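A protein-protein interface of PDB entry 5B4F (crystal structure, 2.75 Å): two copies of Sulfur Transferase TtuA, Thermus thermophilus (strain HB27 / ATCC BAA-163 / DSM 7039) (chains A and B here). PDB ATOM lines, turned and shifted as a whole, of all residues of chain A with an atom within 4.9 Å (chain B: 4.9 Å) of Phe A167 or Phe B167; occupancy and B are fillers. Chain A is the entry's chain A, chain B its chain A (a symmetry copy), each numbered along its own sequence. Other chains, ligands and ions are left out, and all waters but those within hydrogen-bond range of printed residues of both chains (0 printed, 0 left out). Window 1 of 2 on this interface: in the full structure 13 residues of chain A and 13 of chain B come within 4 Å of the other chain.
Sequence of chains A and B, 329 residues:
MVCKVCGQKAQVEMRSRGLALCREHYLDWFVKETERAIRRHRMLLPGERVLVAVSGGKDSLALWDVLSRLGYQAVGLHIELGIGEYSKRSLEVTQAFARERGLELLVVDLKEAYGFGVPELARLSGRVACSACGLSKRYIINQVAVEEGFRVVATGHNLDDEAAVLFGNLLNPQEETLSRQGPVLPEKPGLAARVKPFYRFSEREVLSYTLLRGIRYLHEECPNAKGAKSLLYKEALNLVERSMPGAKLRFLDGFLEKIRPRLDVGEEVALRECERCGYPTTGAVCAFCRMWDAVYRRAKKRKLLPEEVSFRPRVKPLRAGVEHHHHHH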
ATOM      1  N   ALA A 163      24.431  15.396  34.173  1.00  0.00           N
ATOM      2  CA  ALA A 163      24.080  16.730  33.746  1.00  0.00           C
ATOM      3  C   ALA A 163      24.639  17.011  32.356  1.00  0.00           C
ATOM      4  O   ALA A 163      23.951  17.612  31.508  1.00  0.00           O
ATOM      5  CB  ALA A 163      24.585  17.754  34.755  1.00  0.00           C
ATOM      6  N   ALA A 164      25.874  16.563  32.115  1.00  0.00           N
ATOM      7  CA  ALA A 164      26.480  16.716  30.791  1.00  0.00           C
ATOM      8  C   ALA A 164      25.647  15.985  29.744  1.00  0.00           C
ATOM      9  O   ALA A 164      25.393  16.509  28.657  1.00  0.00           O
ATOM     10  CB  ALA A 164      27.894  16.205  30.784  1.00  0.00           C
ATOM     11  N   VAL A 165      25.219  14.776  30.087  1.00  0.00           N
ATOM     12  CA  VAL A 165      24.392  13.976  29.200  1.00  0.00           C
ATOM     13  C   VAL A 165      23.071  14.662  28.926  1.00  0.00           C
ATOM     14  O   VAL A 165      22.673  14.817  27.761  1.00  0.00           O
ATOM     15  CB  VAL A 165      24.116  12.577  29.774  1.00  0.00           C
ATOM     16  CG1 VAL A 165      22.936  11.944  29.049  1.00  0.00           C
ATOM     17  CG2 VAL A 165      25.363  11.719  29.644  1.00  0.00           C
ATOM     18  N   LEU A 166      22.390  15.060  29.994  1.00  0.00           N
ATOM     19  CA  LEU A 166      21.131  15.807  29.880  1.00  0.00           C
ATOM     20  C   LEU A 166      21.280  17.035  28.985  1.00  0.00           C
ATOM     21  O   LEU A 166      20.432  17.313  28.136  1.00  0.00           O
ATOM     22  CB  LEU A 166      20.654  16.224  31.268  1.00  0.00           C
ATOM     23  CG  LEU A 166      19.511  17.222  31.407  1.00  0.00           C
ATOM     24  CD1 LEU A 166      18.263  16.717  30.692  1.00  0.00           C
ATOM     25  CD2 LEU A 166      19.242  17.455  32.895  1.00  0.00           C
ATOM     26  N   PHE A 167      22.372  17.766  29.181  1.00  0.00           N
ATOM     27  CA  PHE A 167      22.638  18.962  28.404  1.00  0.00           C
ATOM     28  C   PHE A 167      22.868  18.623  26.925  1.00  0.00           C
ATOM     29  O   PHE A 167      22.397  19.332  26.023  1.00  0.00           O
ATOM     30  CB  PHE A 167      23.851  19.692  28.987  1.00  0.00           C
ATOM     31  CG  PHE A 167      24.019  21.109  28.496  1.00  0.00           C
ATOM     32  CD1 PHE A 167      22.937  21.832  28.011  1.00  0.00           C
ATOM     33  CD2 PHE A 167      25.267  21.716  28.520  1.00  0.00           C
ATOM     34  CE1 PHE A 167      23.091  23.150  27.560  1.00  0.00           C
ATOM     35  CE2 PHE A 167      25.435  23.033  28.077  1.00  0.00           C
ATOM     36  CZ  PHE A 167      24.340  23.747  27.594  1.00  0.00           C
ATOM     37  N   GLY A 168      23.612  17.548  26.687  1.00  0.00           N
ATOM     38  CA  GLY A 168      23.879  17.088  25.341  1.00  0.00           C
ATOM     39  C   GLY A 168      22.606  16.799  24.571  1.00  0.00           C
ATOM     40  O   GLY A 168      22.506  17.183  23.402  1.00  0.00           O
ATOM     41  N   ASN A 169      21.643  16.142  25.227  1.00  0.00           N
ATOM     42  CA  ASN A 169      20.346  15.812  24.619  1.00  0.00           C
ATOM     43  C   ASN A 169      19.502  17.032  24.279  1.00  0.00           C
ATOM     44  O   ASN A 169      18.820  17.059  23.250  1.00  0.00           O
ATOM     45  CB  ASN A 169      19.509  14.918  25.541  1.00  0.00           C
ATOM     46  CG  ASN A 169      20.241  13.683  26.004  1.00  0.00           C
ATOM     47  OD1 ASN A 169      21.279  13.301  25.449  1.00  0.00           O
ATOM     48  ND2 ASN A 169      19.698  13.039  27.038  1.00  0.00           N
ATOM     49  N   LEU A 170      19.510  18.027  25.162  1.00  0.00           N
ATOM     50  CA  LEU A 170      18.790  19.267  24.890  1.00  0.00           C
ATOM     51  C   LEU A 170      19.361  19.986  23.653  1.00  0.00           C
ATOM     52  O   LEU A 170      18.613  20.597  22.878  1.00  0.00           O
ATOM     53  CB  LEU A 170      18.830  20.190  26.107  1.00  0.00           C
ATOM     54  CG  LEU A 170      18.110  19.691  27.355  1.00  0.00           C
ATOM     55  CD1 LEU A 170      18.109  20.795  28.387  1.00  0.00           C
ATOM     56  CD2 LEU A 170      16.688  19.253  27.028  1.00  0.00           C
ATOM     57  N   LEU A 171      20.681  19.904  23.482  1.00  0.00           N
ATOM     58  CA  LEU A 171      21.359  20.505  22.343  1.00  0.00           C
ATOM     59  C   LEU A 171      21.272  19.599  21.107  1.00  0.00           C
ATOM     60  O   LEU A 171      21.192  20.077  19.974  1.00  0.00           O
ATOM     61  CB  LEU A 171      22.821  20.796  22.687  1.00  0.00           C
ATOM     62  CG  LEU A 171      22.999  21.615  23.972  1.00  0.00           C
ATOM     63  CD1 LEU A 171      24.465  21.740  24.389  1.00  0.00           C
ATOM     64  CD2 LEU A 171      22.379  22.987  23.809  1.00  0.00           C
ATOM     65  N   TYR A 233      30.446  19.809  27.144  1.00  0.00           N
ATOM     66  CA  TYR A 233      29.266  20.081  27.956  1.00  0.00           C
ATOM     67  C   TYR A 233      29.652  20.347  29.395  1.00  0.00           C
ATOM     68  O   TYR A 233      29.037  21.171  30.070  1.00  0.00           O
ATOM     69  CB  TYR A 233      28.277  18.910  27.912  1.00  0.00           C
ATOM     70  CG  TYR A 233      27.839  18.527  26.521  1.00  0.00           C
ATOM     71  CD1 TYR A 233      27.741  19.476  25.511  1.00  0.00           C
ATOM     72  CD2 TYR A 233      27.521  17.215  26.217  1.00  0.00           C
ATOM     73  CE1 TYR A 233      27.338  19.127  24.232  1.00  0.00           C
ATOM     74  CE2 TYR A 233      27.124  16.858  24.947  1.00  0.00           C
ATOM     75  CZ  TYR A 233      27.029  17.819  23.956  1.00  0.00           C
ATOM     76  OH  TYR A 233      26.632  17.472  22.685  1.00  0.00           O
ATOM     77  N   ALA A 236      31.221  23.941  29.895  1.00  0.00           N
ATOM     78  CA  ALA A 236      30.185  24.968  29.825  1.00  0.00           C
ATOM     79  C   ALA A 236      29.341  25.007  31.106  1.00  0.00           C
ATOM     80  O   ALA A 236      29.002  26.075  31.619  1.00  0.00           O
ATOM     81  CB  ALA A 236      29.303  24.727  28.609  1.00  0.00           C
ATOM     82  N   LEU A 237      29.009  23.830  31.619  1.00  0.00           N
ATOM     83  CA  LEU A 237      28.277  23.730  32.869  1.00  0.00           C
ATOM     84  C   LEU A 237      29.165  24.135  34.074  1.00  0.00           C
ATOM     85  O   LEU A 237      28.690  24.771  35.009  1.00  0.00           O
ATOM     86  CB  LEU A 237      27.728  22.309  33.048  1.00  0.00           C
ATOM     87  CG  LEU A 237      26.559  21.802  32.194  1.00  0.00           C
ATOM     88  CD1 LEU A 237      26.355  20.289  32.356  1.00  0.00           C
ATOM     89  CD2 LEU A 237      25.233  22.517  32.480  1.00  0.00           C
ATOM     90  N   VAL A 240      29.397  27.840  34.359  1.00  0.00           N
ATOM     91  CA  VAL A 240      28.240  28.386  35.039  1.00  0.00           C
ATOM     92  C   VAL A 240      28.336  28.093  36.540  1.00  0.00           C
ATOM     93  O   VAL A 240      28.161  28.998  37.351  1.00  0.00           O
ATOM     94  CB  VAL A 240      26.927  27.821  34.449  1.00  0.00           C
ATOM     95  CG1 VAL A 240      25.720  28.354  35.197  1.00  0.00           C
ATOM     96  CG2 VAL A 240      26.825  28.167  32.966  1.00  0.00           C
ATOM     97  N   PHE A 251      19.719  22.141  37.925  1.00  0.00           N
ATOM     98  CA  PHE A 251      19.467  21.756  36.543  1.00  0.00           C
ATOM     99  C   PHE A 251      18.924  20.336  36.450  1.00  0.00           C
ATOM    100  O   PHE A 251      17.804  20.104  35.960  1.00  0.00           O
ATOM    101  CB  PHE A 251      20.769  21.899  35.760  1.00  0.00           C
ATOM    102  CG  PHE A 251      20.693  21.432  34.337  1.00  0.00           C
ATOM    103  CD1 PHE A 251      21.551  20.436  33.881  1.00  0.00           C
ATOM    104  CD2 PHE A 251      19.798  22.005  33.448  1.00  0.00           C
ATOM    105  CE1 PHE A 251      21.509  20.014  32.563  1.00  0.00           C
ATOM    106  CE2 PHE A 251      19.751  21.593  32.137  1.00  0.00           C
ATOM    107  CZ  PHE A 251      20.606  20.593  31.688  1.00  0.00           C
ATOM    108  N   ALA B 163      17.679  31.795  24.199  1.00  0.00           N
ATOM    109  CA  ALA B 163      18.358  30.592  24.619  1.00  0.00           C
ATOM    110  C   ALA B 163      19.005  30.793  25.985  1.00  0.00           C
ATOM    111  O   ALA B 163      18.951  29.895  26.848  1.00  0.00           O
ATOM    112  CB  ALA B 163      19.393  30.183  23.579  1.00  0.00           C
ATOM    113  N   ALA B 164      19.600  31.971  26.188  1.00  0.00           N
ATOM    114  CA  ALA B 164      20.192  32.296  27.488  1.00  0.00           C
ATOM    115  C   ALA B 164      19.122  32.267  28.573  1.00  0.00           C
ATOM    116  O   ALA B 164      19.337  31.728  29.662  1.00  0.00           O
ATOM    117  CB  ALA B 164      20.863  33.640  27.452  1.00  0.00           C
ATOM    118  N   VAL B 165      17.966  32.845  28.263  1.00  0.00           N
ATOM    119  CA  VAL B 165      16.848  32.868  29.190  1.00  0.00           C
ATOM    120  C   VAL B 165      16.374  31.465  29.501  1.00  0.00           C
ATOM    121  O   VAL B 165      16.233  31.094  30.676  1.00  0.00           O
ATOM    122  CB  VAL B 165      15.664  33.684  28.646  1.00  0.00           C
ATOM    123  CG1 VAL B 165      14.399  33.341  29.421  1.00  0.00           C
ATOM    124  CG2 VAL B 165      15.982  35.166  28.744  1.00  0.00           C
ATOM    125  N   LEU B 166      16.117  30.692  28.452  1.00  0.00           N
ATOM    126  CA  LEU B 166      15.723  29.285  28.599  1.00  0.00           C
ATOM    127  C   LEU B 166      16.708  28.510  29.471  1.00  0.00           C
ATOM    128  O   LEU B 166      16.315  27.736  30.345  1.00  0.00           O
ATOM    129  CB  LEU B 166      15.616  28.634  27.223  1.00  0.00           C
ATOM    130  CG  LEU B 166      15.470  27.122  27.111  1.00  0.00           C
ATOM    131  CD1 LEU B 166      14.244  26.639  27.876  1.00  0.00           C
ATOM    132  CD2 LEU B 166      15.384  26.747  25.630  1.00  0.00           C
ATOM    133  N   PHE B 167      17.995  28.729  29.227  1.00  0.00           N
ATOM    134  CA  PHE B 167      19.038  28.056  29.977  1.00  0.00           C
ATOM    135  C   PHE B 167      19.024  28.480  31.451  1.00  0.00           C
ATOM    136  O   PHE B 167      19.203  27.655  32.360  1.00  0.00           O
ATOM    137  CB  PHE B 167      20.400  28.353  29.341  1.00  0.00           C
ATOM    138  CG  PHE B 167      21.515  27.449  29.806  1.00  0.00           C
ATOM    139  CD1 PHE B 167      21.245  26.186  30.319  1.00  0.00           C
ATOM    140  CD2 PHE B 167      22.835  27.867  29.729  1.00  0.00           C
ATOM    141  CE1 PHE B 167      22.280  25.343  30.745  1.00  0.00           C
ATOM    142  CE2 PHE B 167      23.880  27.035  30.148  1.00  0.00           C
ATOM    143  CZ  PHE B 167      23.594  25.770  30.659  1.00  0.00           C
ATOM    144  N   GLY B 168      18.831  29.776  31.679  1.00  0.00           N
ATOM    145  CA  GLY B 168      18.755  30.313  33.020  1.00  0.00           C
ATOM    146  C   GLY B 168      17.662  29.657  33.839  1.00  0.00           C
ATOM    147  O   GLY B 168      17.895  29.325  35.005  1.00  0.00           O
ATOM    148  N   ASN B 169      16.489  29.461  33.227  1.00  0.00           N
ATOM    149  CA  ASN B 169      15.343  28.815  33.884  1.00  0.00           C
ATOM    150  C   ASN B 169      15.584  27.353  34.237  1.00  0.00           C
ATOM    151  O   ASN B 169      15.144  26.879  35.288  1.00  0.00           O
ATOM    152  CB  ASN B 169      14.088  28.874  33.005  1.00  0.00           C
ATOM    153  CG  ASN B 169      13.752  30.267  32.534  1.00  0.00           C
ATOM    154  OD1 ASN B 169      14.260  31.267  33.057  1.00  0.00           O
ATOM    155  ND2 ASN B 169      12.879  30.344  31.529  1.00  0.00           N
ATOM    156  N   LEU B 170      16.243  26.625  33.340  1.00  0.00           N
ATOM    157  CA  LEU B 170      16.585  25.234  33.620  1.00  0.00           C
ATOM    158  C   LEU B 170      17.538  25.124  34.825  1.00  0.00           C
ATOM    159  O   LEU B 170      17.444  24.177  35.618  1.00  0.00           O
ATOM    160  CB  LEU B 170      17.207  24.575  32.389  1.00  0.00           C
ATOM    161  CG  LEU B 170      16.298  24.425  31.174  1.00  0.00           C
ATOM    162  CD1 LEU B 170      17.021  23.608  30.128  1.00  0.00           C
ATOM    163  CD2 LEU B 170      14.978  23.767  31.557  1.00  0.00           C
ATOM    164  N   LEU B 171      18.444  26.095  34.951  1.00  0.00           N
ATOM    165  CA  LEU B 171      19.388  26.141  36.057  1.00  0.00           C
ATOM    166  C   LEU B 171      18.745  26.757  37.308  1.00  0.00           C
ATOM    167  O   LEU B 171      19.056  26.371  38.437  1.00  0.00           O
ATOM    168  CB  LEU B 171      20.636  26.933  35.658  1.00  0.00           C
ATOM    169  CG  LEU B 171      21.283  26.444  34.356  1.00  0.00           C
ATOM    170  CD1 LEU B 171      22.416  27.356  33.886  1.00  0.00           C
ATOM    171  CD2 LEU B 171      21.784  25.024  34.521  1.00  0.00           C
ATOM    172  N   TYR B 233      25.322  32.836  30.949  1.00  0.00           N
ATOM    173  CA  TYR B 233      24.626  31.815  30.175  1.00  0.00           C
ATOM    174  C   TYR B 233      25.038  31.868  28.720  1.00  0.00           C
ATOM    175  O   TYR B 233      25.136  30.836  28.056  1.00  0.00           O
ATOM    176  CB  TYR B 233      23.105  31.983  30.271  1.00  0.00           C
ATOM    177  CG  TYR B 233      22.572  31.979  31.681  1.00  0.00           C
ATOM    178  CD1 TYR B 233      23.191  31.238  32.681  1.00  0.00           C
ATOM    179  CD2 TYR B 233      21.450  32.716  32.015  1.00  0.00           C
ATOM    180  CE1 TYR B 233      22.704  31.231  33.978  1.00  0.00           C
ATOM    181  CE2 TYR B 233      20.961  32.719  33.303  1.00  0.00           C
ATOM    182  CZ  TYR B 233      21.589  31.971  34.283  1.00  0.00           C
ATOM    183  OH  TYR B 233      21.107  31.967  35.573  1.00  0.00           O
ATOM    184  N   ALA B 236      28.632  30.335  28.114  1.00  0.00           N
ATOM    185  CA  ALA B 236      28.591  28.878  28.207  1.00  0.00           C
ATOM    186  C   ALA B 236      27.960  28.250  26.955  1.00  0.00           C
ATOM    187  O   ALA B 236      28.433  27.236  26.440  1.00  0.00           O
ATOM    188  CB  ALA B 236      27.828  28.463  29.456  1.00  0.00           C
ATOM    189  N   LEU B 237      26.892  28.868  26.471  1.00  0.00           N
ATOM    190  CA  LEU B 237      26.249  28.419  25.250  1.00  0.00           C
ATOM    191  C   LEU B 237      27.129  28.719  24.008  1.00  0.00           C
ATOM    192  O   LEU B 237      27.190  27.918  23.082  1.00  0.00           O
ATOM    193  CB  LEU B 237      24.867  29.069  25.110  1.00  0.00           C
ATOM    194  CG  LEU B 237      23.701  28.643  26.012  1.00  0.00           C
ATOM    195  CD1 LEU B 237      22.506  29.598  25.879  1.00  0.00           C
ATOM    196  CD2 LEU B 237      23.222  27.208  25.762  1.00  0.00           C
ATOM    197  N   VAL B 240      29.837  26.189  23.663  1.00  0.00           N
ATOM    198  CA  VAL B 240      29.352  24.987  23.016  1.00  0.00           C
ATOM    199  C   VAL B 240      29.166  25.244  21.518  1.00  0.00           C
ATOM    200  O   VAL B 240      29.634  24.457  20.701  1.00  0.00           O
ATOM    201  CB  VAL B 240      28.033  24.501  23.660  1.00  0.00           C
ATOM    202  CG1 VAL B 240      27.499  23.272  22.948  1.00  0.00           C
ATOM    203  CG2 VAL B 240      28.249  24.201  25.142  1.00  0.00           C
ATOM    204  N   PHE B 251      18.779  23.607  20.521  1.00  0.00           N
ATOM    205  CA  PHE B 251      18.380  23.732  21.916  1.00  0.00           C
ATOM    206  C   PHE B 251      17.012  24.389  22.048  1.00  0.00           C
ATOM    207  O   PHE B 251      16.058  23.794  22.580  1.00  0.00           O
ATOM    208  CB  PHE B 251      19.448  24.537  22.651  1.00  0.00           C
ATOM    209  CG  PHE B 251      19.121  24.842  24.082  1.00  0.00           C
ATOM    210  CD1 PHE B 251      19.073  26.161  24.521  1.00  0.00           C
ATOM    211  CD2 PHE B 251      18.900  23.823  24.994  1.00  0.00           C
ATOM    212  CE1 PHE B 251      18.800  26.458  25.846  1.00  0.00           C
ATOM    213  CE2 PHE B 251      18.628  24.108  26.311  1.00  0.00           C
ATOM    214  CZ  PHE B 251      18.574  25.429  26.744  1.00  0.00           C
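Of the 14 printed residues of chain B, 6 touch a printed residue of chain A. Hydrophobic or aromatic side chains of chain B within 4 Å of the printed part of chain A: Phe B167, Leu B170, Leu B171, Ala B236, Val B240 and Phe B251. Along chain B the printed residues that touch a printed residue of chain A span positions 167 to 251. Printed residues of chain A that touch a printed residue of chain B: Phe A167, Leu A170, Leu A171, Ala A236, Val A240 and Phe A251. Hydrophobic or aromatic side chains of chain A that line the printed part of chain B: Phe A167, Leu A170, Leu A171, Ala A236, Val A240 and Phe A251. Among the printed residues, no Asp or Glu carboxylate lies within 4 Å of a Lys or Arg side-chain nitrogen of the other chain.
Among the printed residues, merely in contact across the chains: Leu A170 with Phe B251 (3.3 Å), Phe A251 with Leu B170 (3.3 Å), Ala A236 with Ala B236 (3.4 Å), Leu A170 with Leu B170 (3.5 Å), Phe A251 with Leu B171 (3.5 Å), Leu A171 with Phe B251 (3.5 Å), Ala A236 with Val B240 (3.7 Å), Val A240 with Ala B236 (3.7 Å), Leu A171 with Val B240 (3.7 Å), Val A240 with Leu B171 (3.7 Å) and Phe A167 with Phe B167 (3.7 Å).
Of chain B, only Phe B167 (3.7 Å) comes within 4 Å of Phe A167. Printed residues of chain B within 4 Å of Leu A170: Leu B170 and Phe B251. Of chain A, only Phe A167 comes within 4 Å of Phe B167. Printed residues of chain A within 4 Å of Val B240: Leu A171 (3.7 Å) and Ala A236 (3.7 Å). The nearest residue of chain B that does not touch Phe A167 is Leu B237 (4.1 Å). The nearest residue of chain A that does not touch Phe B167 is Leu A237 (4.1 Å).
Leu A170 touches its own counterpart, Leu B170. Leu A171 touches Val B240, and with the chains exchanged Val A240 touches Leu B171. Leu A171 touches Phe B251, and with the chains exchanged Phe A251 touches Leu B171. Ala B236 touches its own counterpart, Ala A236. Positions printed for both chains: 163, 164, 165, 166, 167, 168, 169, 170, 171, 233, 236, 237, 240 and 251.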
